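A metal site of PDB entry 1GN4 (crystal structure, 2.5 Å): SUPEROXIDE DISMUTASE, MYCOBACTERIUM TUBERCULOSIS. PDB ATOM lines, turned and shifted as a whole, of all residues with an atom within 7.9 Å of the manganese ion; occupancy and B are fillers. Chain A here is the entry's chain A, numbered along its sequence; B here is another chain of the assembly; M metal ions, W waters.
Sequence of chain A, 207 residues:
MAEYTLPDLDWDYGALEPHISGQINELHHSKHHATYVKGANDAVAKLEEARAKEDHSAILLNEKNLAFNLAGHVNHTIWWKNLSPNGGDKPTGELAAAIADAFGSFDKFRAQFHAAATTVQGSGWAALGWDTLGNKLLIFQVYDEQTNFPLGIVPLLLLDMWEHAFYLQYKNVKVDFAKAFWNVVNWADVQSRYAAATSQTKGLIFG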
ATOM      1  N   HIS A  28      13.209  -5.755  -2.018  1.00  0.00           N
ATOM      2  CA  HIS A  28      12.552  -7.021  -1.623  1.00  0.00           C
ATOM      3  C   HIS A  28      11.305  -7.185  -2.462  1.00  0.00           C
ATOM      4  O   HIS A  28      11.122  -8.169  -3.188  1.00  0.00           O
ATOM      5  CB  HIS A  28      12.275  -7.056  -0.111  1.00  0.00           C
ATOM      6  CG  HIS A  28      12.118  -8.388   0.552  1.00  0.00           C
ATOM      7  ND1 HIS A  28      11.737  -8.536   1.878  1.00  0.00           N
ATOM      8  CD2 HIS A  28      12.281  -9.656   0.088  1.00  0.00           C
ATOM      9  CE1 HIS A  28      11.658  -9.830   2.184  1.00  0.00           C
ATOM     10  NE2 HIS A  28      11.983 -10.536   1.107  1.00  0.00           N
ATOM     11  N   HIS A  29      10.457  -6.173  -2.377  1.00  0.00           N
ATOM     12  CA  HIS A  29       9.165  -6.272  -3.137  1.00  0.00           C
ATOM     13  C   HIS A  29       9.353  -6.253  -4.610  1.00  0.00           C
ATOM     14  O   HIS A  29       9.035  -7.177  -5.371  1.00  0.00           O
ATOM     15  CB  HIS A  29       8.367  -5.078  -2.746  1.00  0.00           C
ATOM     16  CG  HIS A  29       6.995  -5.006  -3.343  1.00  0.00           C
ATOM     17  ND1 HIS A  29       6.686  -4.144  -4.384  1.00  0.00           N
ATOM     18  CD2 HIS A  29       5.826  -5.622  -3.018  1.00  0.00           C
ATOM     19  CE1 HIS A  29       5.412  -4.277  -4.701  1.00  0.00           C
ATOM     20  NE2 HIS A  29       4.862  -5.178  -3.895  1.00  0.00           N
ATOM     21  N   HIS A  32      12.964  -9.056  -5.625  1.00  0.00           N
ATOM     22  CA  HIS A  32      12.841 -10.479  -5.230  1.00  0.00           C
ATOM     23  C   HIS A  32      11.456 -10.967  -5.444  1.00  0.00           C
ATOM     24  O   HIS A  32      11.198 -11.933  -6.203  1.00  0.00           O
ATOM     25  CB  HIS A  32      13.324 -10.686  -3.732  1.00  0.00           C
ATOM     26  CG  HIS A  32      14.789 -10.331  -3.655  1.00  0.00           C
ATOM     27  ND1 HIS A  32      15.777 -11.122  -4.195  1.00  0.00           N
ATOM     28  CD2 HIS A  32      15.409  -9.259  -3.118  1.00  0.00           C
ATOM     29  CE1 HIS A  32      16.963 -10.552  -3.974  1.00  0.00           C
ATOM     30  NE2 HIS A  32      16.761  -9.421  -3.323  1.00  0.00           N
ATOM     31  N   HIS A  33      10.497 -10.290  -4.807  1.00  0.00           N
ATOM     32  CA  HIS A  33       9.085 -10.851  -5.035  1.00  0.00           C
ATOM     33  C   HIS A  33       8.607 -10.859  -6.468  1.00  0.00           C
ATOM     34  O   HIS A  33       7.953 -11.803  -6.938  1.00  0.00           O
ATOM     35  CB  HIS A  33       8.241  -9.967  -4.073  1.00  0.00           C
ATOM     36  CG  HIS A  33       6.902 -10.609  -3.862  1.00  0.00           C
ATOM     37  ND1 HIS A  33       6.039 -10.226  -2.865  1.00  0.00           N
ATOM     38  CD2 HIS A  33       6.265 -11.569  -4.581  1.00  0.00           C
ATOM     39  CE1 HIS A  33       4.941 -10.952  -2.944  1.00  0.00           C
ATOM     40  NE2 HIS A  33       5.036 -11.765  -3.981  1.00  0.00           N
ATOM     41  N   TYR A  36       9.902 -13.994  -8.177  1.00  0.00           N
ATOM     42  CA  TYR A  36       9.245 -15.320  -7.936  1.00  0.00           C
ATOM     43  C   TYR A  36       7.905 -15.264  -8.736  1.00  0.00           C
ATOM     44  O   TYR A  36       7.498 -16.274  -9.312  1.00  0.00           O
ATOM     45  CB  TYR A  36       8.867 -15.212  -6.430  1.00  0.00           C
ATOM     46  CG  TYR A  36      10.004 -15.550  -5.460  1.00  0.00           C
ATOM     47  CD1 TYR A  36      10.781 -16.681  -5.622  1.00  0.00           C
ATOM     48  CD2 TYR A  36      10.274 -14.775  -4.339  1.00  0.00           C
ATOM     49  CE1 TYR A  36      11.783 -17.036  -4.709  1.00  0.00           C
ATOM     50  CE2 TYR A  36      11.267 -15.092  -3.410  1.00  0.00           C
ATOM     51  CZ  TYR A  36      12.023 -16.227  -3.612  1.00  0.00           C
ATOM     52  OH  TYR A  36      13.037 -16.588  -2.754  1.00  0.00           O
ATOM     53  N   GLY A  72       7.671 -19.065  -2.985  1.00  0.00           N
ATOM     54  CA  GLY A  72       8.147 -17.741  -2.567  1.00  0.00           C
ATOM     55  C   GLY A  72       7.022 -16.737  -2.760  1.00  0.00           C
ATOM     56  O   GLY A  72       6.760 -15.816  -1.965  1.00  0.00           O
ATOM     57  N   ASN A  75       4.632 -16.954   0.074  1.00  0.00           N
ATOM     58  CA  ASN A  75       5.207 -16.471   1.375  1.00  0.00           C
ATOM     59  C   ASN A  75       5.358 -14.995   1.446  1.00  0.00           C
ATOM     60  O   ASN A  75       5.102 -14.329   2.455  1.00  0.00           O
ATOM     61  CB  ASN A  75       6.656 -17.120   1.447  1.00  0.00           C
ATOM     62  CG  ASN A  75       6.640 -18.594   1.710  1.00  0.00           C
ATOM     63  OD1 ASN A  75       5.605 -19.248   1.908  1.00  0.00           O
ATOM     64  ND2 ASN A  75       7.827 -19.179   1.697  1.00  0.00           N
ATOM     65  N   HIS A  76       5.801 -14.383   0.345  1.00  0.00           N
ATOM     66  CA  HIS A  76       5.957 -12.858   0.471  1.00  0.00           C
ATOM     67  C   HIS A  76       4.640 -12.153   0.496  1.00  0.00           C
ATOM     68  O   HIS A  76       4.463 -11.141   1.185  1.00  0.00           O
ATOM     69  CB  HIS A  76       6.798 -12.482  -0.747  1.00  0.00           C
ATOM     70  CG  HIS A  76       8.243 -12.859  -0.556  1.00  0.00           C
ATOM     71  ND1 HIS A  76       8.708 -14.128  -0.802  1.00  0.00           N
ATOM     72  CD2 HIS A  76       9.319 -12.142  -0.155  1.00  0.00           C
ATOM     73  CE1 HIS A  76      10.014 -14.170  -0.557  1.00  0.00           C
ATOM     74  NE2 HIS A  76      10.417 -12.985  -0.135  1.00  0.00           N
ATOM     75  N   TRP A  79       3.648 -12.124   3.917  1.00  0.00           N
ATOM     76  CA  TRP A  79       4.638 -11.333   4.743  1.00  0.00           C
ATOM     77  C   TRP A  79       4.258  -9.833   4.645  1.00  0.00           C
ATOM     78  O   TRP A  79       4.262  -9.118   5.655  1.00  0.00           O
ATOM     79  CB  TRP A  79       6.017 -11.520   4.132  1.00  0.00           C
ATOM     80  CG  TRP A  79       7.150 -10.550   4.398  1.00  0.00           C
ATOM     81  CD1 TRP A  79       7.755  -9.730   3.481  1.00  0.00           C
ATOM     82  CD2 TRP A  79       7.909 -10.425   5.614  1.00  0.00           C
ATOM     83  NE1 TRP A  79       8.819  -9.077   4.081  1.00  0.00           N
ATOM     84  CE2 TRP A  79       8.911  -9.470   5.395  1.00  0.00           C
ATOM     85  CE3 TRP A  79       7.816 -11.039   6.871  1.00  0.00           C
ATOM     86  CZ2 TRP A  79       9.834  -9.100   6.391  1.00  0.00           C
ATOM     87  CZ3 TRP A  79       8.720 -10.676   7.856  1.00  0.00           C
ATOM     88  CH2 TRP A  79       9.721  -9.729   7.616  1.00  0.00           C
ATOM     89  N   TRP A  80       3.936  -9.342   3.446  1.00  0.00           N
ATOM     90  CA  TRP A  80       3.561  -7.845   3.415  1.00  0.00           C
ATOM     91  C   TRP A  80       2.300  -7.664   4.242  1.00  0.00           C
ATOM     92  O   TRP A  80       2.140  -6.666   4.972  1.00  0.00           O
ATOM     93  CB  TRP A  80       3.331  -7.581   1.916  1.00  0.00           C
ATOM     94  CG  TRP A  80       4.545  -7.794   1.082  1.00  0.00           C
ATOM     95  CD1 TRP A  80       4.608  -8.600  -0.065  1.00  0.00           C
ATOM     96  CD2 TRP A  80       5.853  -7.274   1.268  1.00  0.00           C
ATOM     97  NE1 TRP A  80       5.883  -8.550  -0.591  1.00  0.00           N
ATOM     98  CE2 TRP A  80       6.662  -7.766   0.219  1.00  0.00           C
ATOM     99  CE3 TRP A  80       6.435  -6.428   2.204  1.00  0.00           C
ATOM    100  CZ2 TRP A  80       7.978  -7.371   0.055  1.00  0.00           C
ATOM    101  CZ3 TRP A  80       7.752  -6.108   2.069  1.00  0.00           C
ATOM    102  CH2 TRP A  80       8.541  -6.579   1.013  1.00  0.00           C
ATOM    103  N   GLY A 124      15.798 -19.383   4.975  1.00  0.00           N
ATOM    104  CA  GLY A 124      14.622 -20.025   5.563  1.00  0.00           C
ATOM    105  C   GLY A 124      13.730 -18.994   6.225  1.00  0.00           C
ATOM    106  O   GLY A 124      14.127 -17.828   6.131  1.00  0.00           O
ATOM    107  N   TRP A 125      12.655 -19.442   6.860  1.00  0.00           N
ATOM    108  CA  TRP A 125      11.715 -18.575   7.599  1.00  0.00           C
ATOM    109  C   TRP A 125      11.163 -19.244   8.899  1.00  0.00           C
ATOM    110  O   TRP A 125      11.353 -20.436   9.124  1.00  0.00           O
ATOM    111  CB  TRP A 125      10.247 -18.704   6.825  1.00  0.00           C
ATOM    112  CG  TRP A 125      10.363 -18.126   5.423  1.00  0.00           C
ATOM    113  CD1 TRP A 125      10.992 -18.506   4.281  1.00  0.00           C
ATOM    114  CD2 TRP A 125       9.624 -16.939   5.087  1.00  0.00           C
ATOM    115  NE1 TRP A 125      10.714 -17.614   3.243  1.00  0.00           N
ATOM    116  CE2 TRP A 125       9.929 -16.611   3.757  1.00  0.00           C
ATOM    117  CE3 TRP A 125       8.845 -16.077   5.861  1.00  0.00           C
ATOM    118  CZ2 TRP A 125       9.370 -15.509   3.133  1.00  0.00           C
ATOM    119  CZ3 TRP A 125       8.326 -14.965   5.238  1.00  0.00           C
ATOM    120  CH2 TRP A 125       8.560 -14.725   3.886  1.00  0.00           C
ATOM    121  N   ASP A 144      14.496 -22.650   2.755  1.00  0.00           N
ATOM    122  CA  ASP A 144      14.174 -22.082   1.433  1.00  0.00           C
ATOM    123  C   ASP A 144      12.826 -21.409   1.403  1.00  0.00           C
ATOM    124  O   ASP A 144      12.570 -20.468   2.154  1.00  0.00           O
ATOM    125  CB  ASP A 144      14.597 -22.840   0.295  1.00  0.00           C
ATOM    126  CG  ASP A 144      15.962 -23.509   0.473  1.00  0.00           C
ATOM    127  OD1 ASP A 144      16.745 -22.837   1.178  1.00  0.00           O
ATOM    128  OD2 ASP A 144      16.207 -24.613  -0.033  1.00  0.00           O
ATOM    129  N   GLU A 145      11.911 -21.835   0.523  1.00  0.00           N
ATOM    130  CA  GLU A 145      10.569 -21.058   0.587  1.00  0.00           C
ATOM    131  C   GLU A 145       9.608 -22.280   0.679  1.00  0.00           C
ATOM    132  O   GLU A 145       8.507 -22.133   1.217  1.00  0.00           O
ATOM    133  CB  GLU A 145      10.337 -20.548  -0.840  1.00  0.00           C
ATOM    134  CG  GLU A 145      11.269 -19.381  -1.305  1.00  0.00           C
ATOM    135  CD  GLU A 145      11.030 -18.189  -0.428  1.00  0.00           C
ATOM    136  OE1 GLU A 145      10.117 -18.256   0.447  1.00  0.00           O
ATOM    137  OE2 GLU A 145      11.726 -17.166  -0.581  1.00  0.00           O
ATOM    138  N   ASP A 160      10.688 -13.878   7.558  1.00  0.00           N
ATOM    139  CA  ASP A 160      11.626 -14.173   6.474  1.00  0.00           C
ATOM    140  C   ASP A 160      13.059 -14.085   6.990  1.00  0.00           C
ATOM    141  O   ASP A 160      13.477 -12.977   7.342  1.00  0.00           O
ATOM    142  CB  ASP A 160      11.521 -13.021   5.429  1.00  0.00           C
ATOM    143  CG  ASP A 160      12.207 -13.420   4.141  1.00  0.00           C
ATOM    144  OD1 ASP A 160      13.056 -14.305   4.335  1.00  0.00           O
ATOM    145  OD2 ASP A 160      11.887 -12.875   3.061  1.00  0.00           O
ATOM    146  N   MET A 161      13.755 -15.212   7.050  1.00  0.00           N
ATOM    147  CA  MET A 161      15.130 -15.285   7.539  1.00  0.00           C
ATOM    148  C   MET A 161      16.171 -15.300   6.452  1.00  0.00           C
ATOM    149  O   MET A 161      17.374 -15.540   6.694  1.00  0.00           O
ATOM    150  CB  MET A 161      15.419 -15.935   8.738  1.00  0.00           C
ATOM    151  CG  MET A 161      14.455 -15.721   9.961  1.00  0.00           C
ATOM    152  SD  MET A 161      15.099 -14.113  10.607  1.00  0.00           S
ATOM    153  CE  MET A 161      16.779 -14.050  10.866  1.00  0.00           C
ATOM    154  N   TRP A 162      15.718 -15.067   5.227  1.00  0.00           N
ATOM    155  CA  TRP A 162      16.657 -15.031   4.070  1.00  0.00           C
ATOM    156  C   TRP A 162      17.557 -13.797   4.356  1.00  0.00           C
ATOM    157  O   TRP A 162      17.106 -12.869   5.022  1.00  0.00           O
ATOM    158  CB  TRP A 162      15.869 -14.943   2.763  1.00  0.00           C
ATOM    159  CG  TRP A 162      15.389 -16.222   2.181  1.00  0.00           C
ATOM    160  CD1 TRP A 162      14.518 -17.080   2.826  1.00  0.00           C
ATOM    161  CD2 TRP A 162      15.685 -16.803   0.904  1.00  0.00           C
ATOM    162  NE1 TRP A 162      14.235 -18.139   1.975  1.00  0.00           N
ATOM    163  CE2 TRP A 162      14.937 -17.993   0.807  1.00  0.00           C
ATOM    164  CE3 TRP A 162      16.469 -16.415  -0.189  1.00  0.00           C
ATOM    165  CZ2 TRP A 162      15.018 -18.853  -0.295  1.00  0.00           C
ATOM    166  CZ3 TRP A 162      16.506 -17.245  -1.332  1.00  0.00           C
ATOM    167  CH2 TRP A 162      15.752 -18.426  -1.380  1.00  0.00           C
ATOM    168  N   GLU A 163      18.781 -13.837   3.828  1.00  0.00           N
ATOM    169  CA  GLU A 163      19.733 -12.739   4.057  1.00  0.00           C
ATOM    170  C   GLU A 163      19.273 -11.427   3.537  1.00  0.00           C
ATOM    171  O   GLU A 163      19.390 -10.337   4.123  1.00  0.00           O
ATOM    172  CB  GLU A 163      21.163 -13.109   3.757  1.00  0.00           C
ATOM    173  CG  GLU A 163      21.856 -14.028   4.807  1.00  0.00           C
ATOM    174  CD  GLU A 163      23.188 -14.577   4.313  1.00  0.00           C
ATOM    175  OE1 GLU A 163      23.516 -14.571   3.105  1.00  0.00           O
ATOM    176  OE2 GLU A 163      23.979 -15.005   5.180  1.00  0.00           O
ATOM    177  N   HIS A 164      18.764 -11.472   2.318  1.00  0.00           N
ATOM    178  CA  HIS A 164      18.237 -10.291   1.622  1.00  0.00           C
ATOM    179  C   HIS A 164      17.181  -9.688   2.505  1.00  0.00           C
ATOM    180  O   HIS A 164      16.851  -8.510   2.397  1.00  0.00           O
ATOM    181  CB  HIS A 164      17.764 -10.868   0.249  1.00  0.00           C
ATOM    182  CG  HIS A 164      16.504 -11.653   0.250  1.00  0.00           C
ATOM    183  ND1 HIS A 164      16.380 -12.804  -0.514  1.00  0.00           N
ATOM    184  CD2 HIS A 164      15.281 -11.469   0.831  1.00  0.00           C
ATOM    185  CE1 HIS A 164      15.150 -13.305  -0.365  1.00  0.00           C
ATOM    186  NE2 HIS A 164      14.445 -12.510   0.425  1.00  0.00           N
ATOM    187  N   ALA A 165      16.631 -10.421   3.492  1.00  0.00           N
ATOM    188  CA  ALA A 165      15.603  -9.592   4.288  1.00  0.00           C
ATOM    189  C   ALA A 165      16.313  -8.720   5.278  1.00  0.00           C
ATOM    190  O   ALA A 165      15.666  -7.905   5.999  1.00  0.00           O
ATOM    191  CB  ALA A 165      14.705 -10.603   5.072  1.00  0.00           C
ATOM    192  N   GLU B 163      23.934 -15.025  -0.344  1.00  0.00           N
ATOM    193  CA  GLU B 163      23.705 -13.571  -0.412  1.00  0.00           C
ATOM    194  C   GLU B 163      24.759 -12.674   0.185  1.00  0.00           C
ATOM    195  O   GLU B 163      25.076 -11.584  -0.333  1.00  0.00           O
ATOM    196  CB  GLU B 163      22.292 -13.168  -0.199  1.00  0.00           C
ATOM    197  CG  GLU B 163      21.256 -13.499  -1.317  1.00  0.00           C
ATOM    198  CD  GLU B 163      19.894 -13.519  -0.654  1.00  0.00           C
ATOM    199  OE1 GLU B 163      19.791 -13.536   0.604  1.00  0.00           O
ATOM    200  OE2 GLU B 163      18.822 -13.471  -1.292  1.00  0.00           O
HETATM  201 MN    MN M   1      12.407 -12.827   1.106  1.00  0.00          MN
HETATM  202  O   HOH W   1      12.662 -15.015   1.095  1.00  0.00           O
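O of Gly 72 is in hydrogen-bond range of ND1 of His 76. The backbone carbonyl oxygen (O) of His 76 lies close to the indole nitrogen (NE1) of Trp 80 (3.4 Å). A ring nitrogen (ND1) of His 164 sits at hydrogen-bond distance from the side-chain carboxylate (OE2) of Glu 163 of chain B (2.6 Å). N of Trp 162 lies within hydrogen-bond range of OD1 of Asp 160 (2.9 Å). The backbone NH (N) of His 33 lies within hydrogen-bond range of the backbone carbonyl oxygen (O) of His 28.
Four residues have an atom within 4 Å of the manganese ion: His 28, His 76, Asp 160 and His 164. Along chain A the residues within 4 Å of the manganese ion span positions 28 to 164. The nearest printed residue that does not touch the manganese ion is Trp 162 (4.4 Å).
The side-chain carboxylate (OD2) of Asp 160 binds the manganese ion (2.0 Å). The manganese ion is bound by a ring nitrogen (NE2) of His 164 (2.2 Å). Water W1 is bound to the manganese ion. NE2 of His 28 binds the manganese ion, at 2.3 Å. NE2 of His 76 binds the manganese ion (2.4 Å). The manganese ion has five donor atoms within binding distance.
Water W1 bridges the side-chain carboxylate (OE2) of Glu 145 (2.9 Å) and the side-chain carboxylate (OD1) of Asp 160 (3.3 Å).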
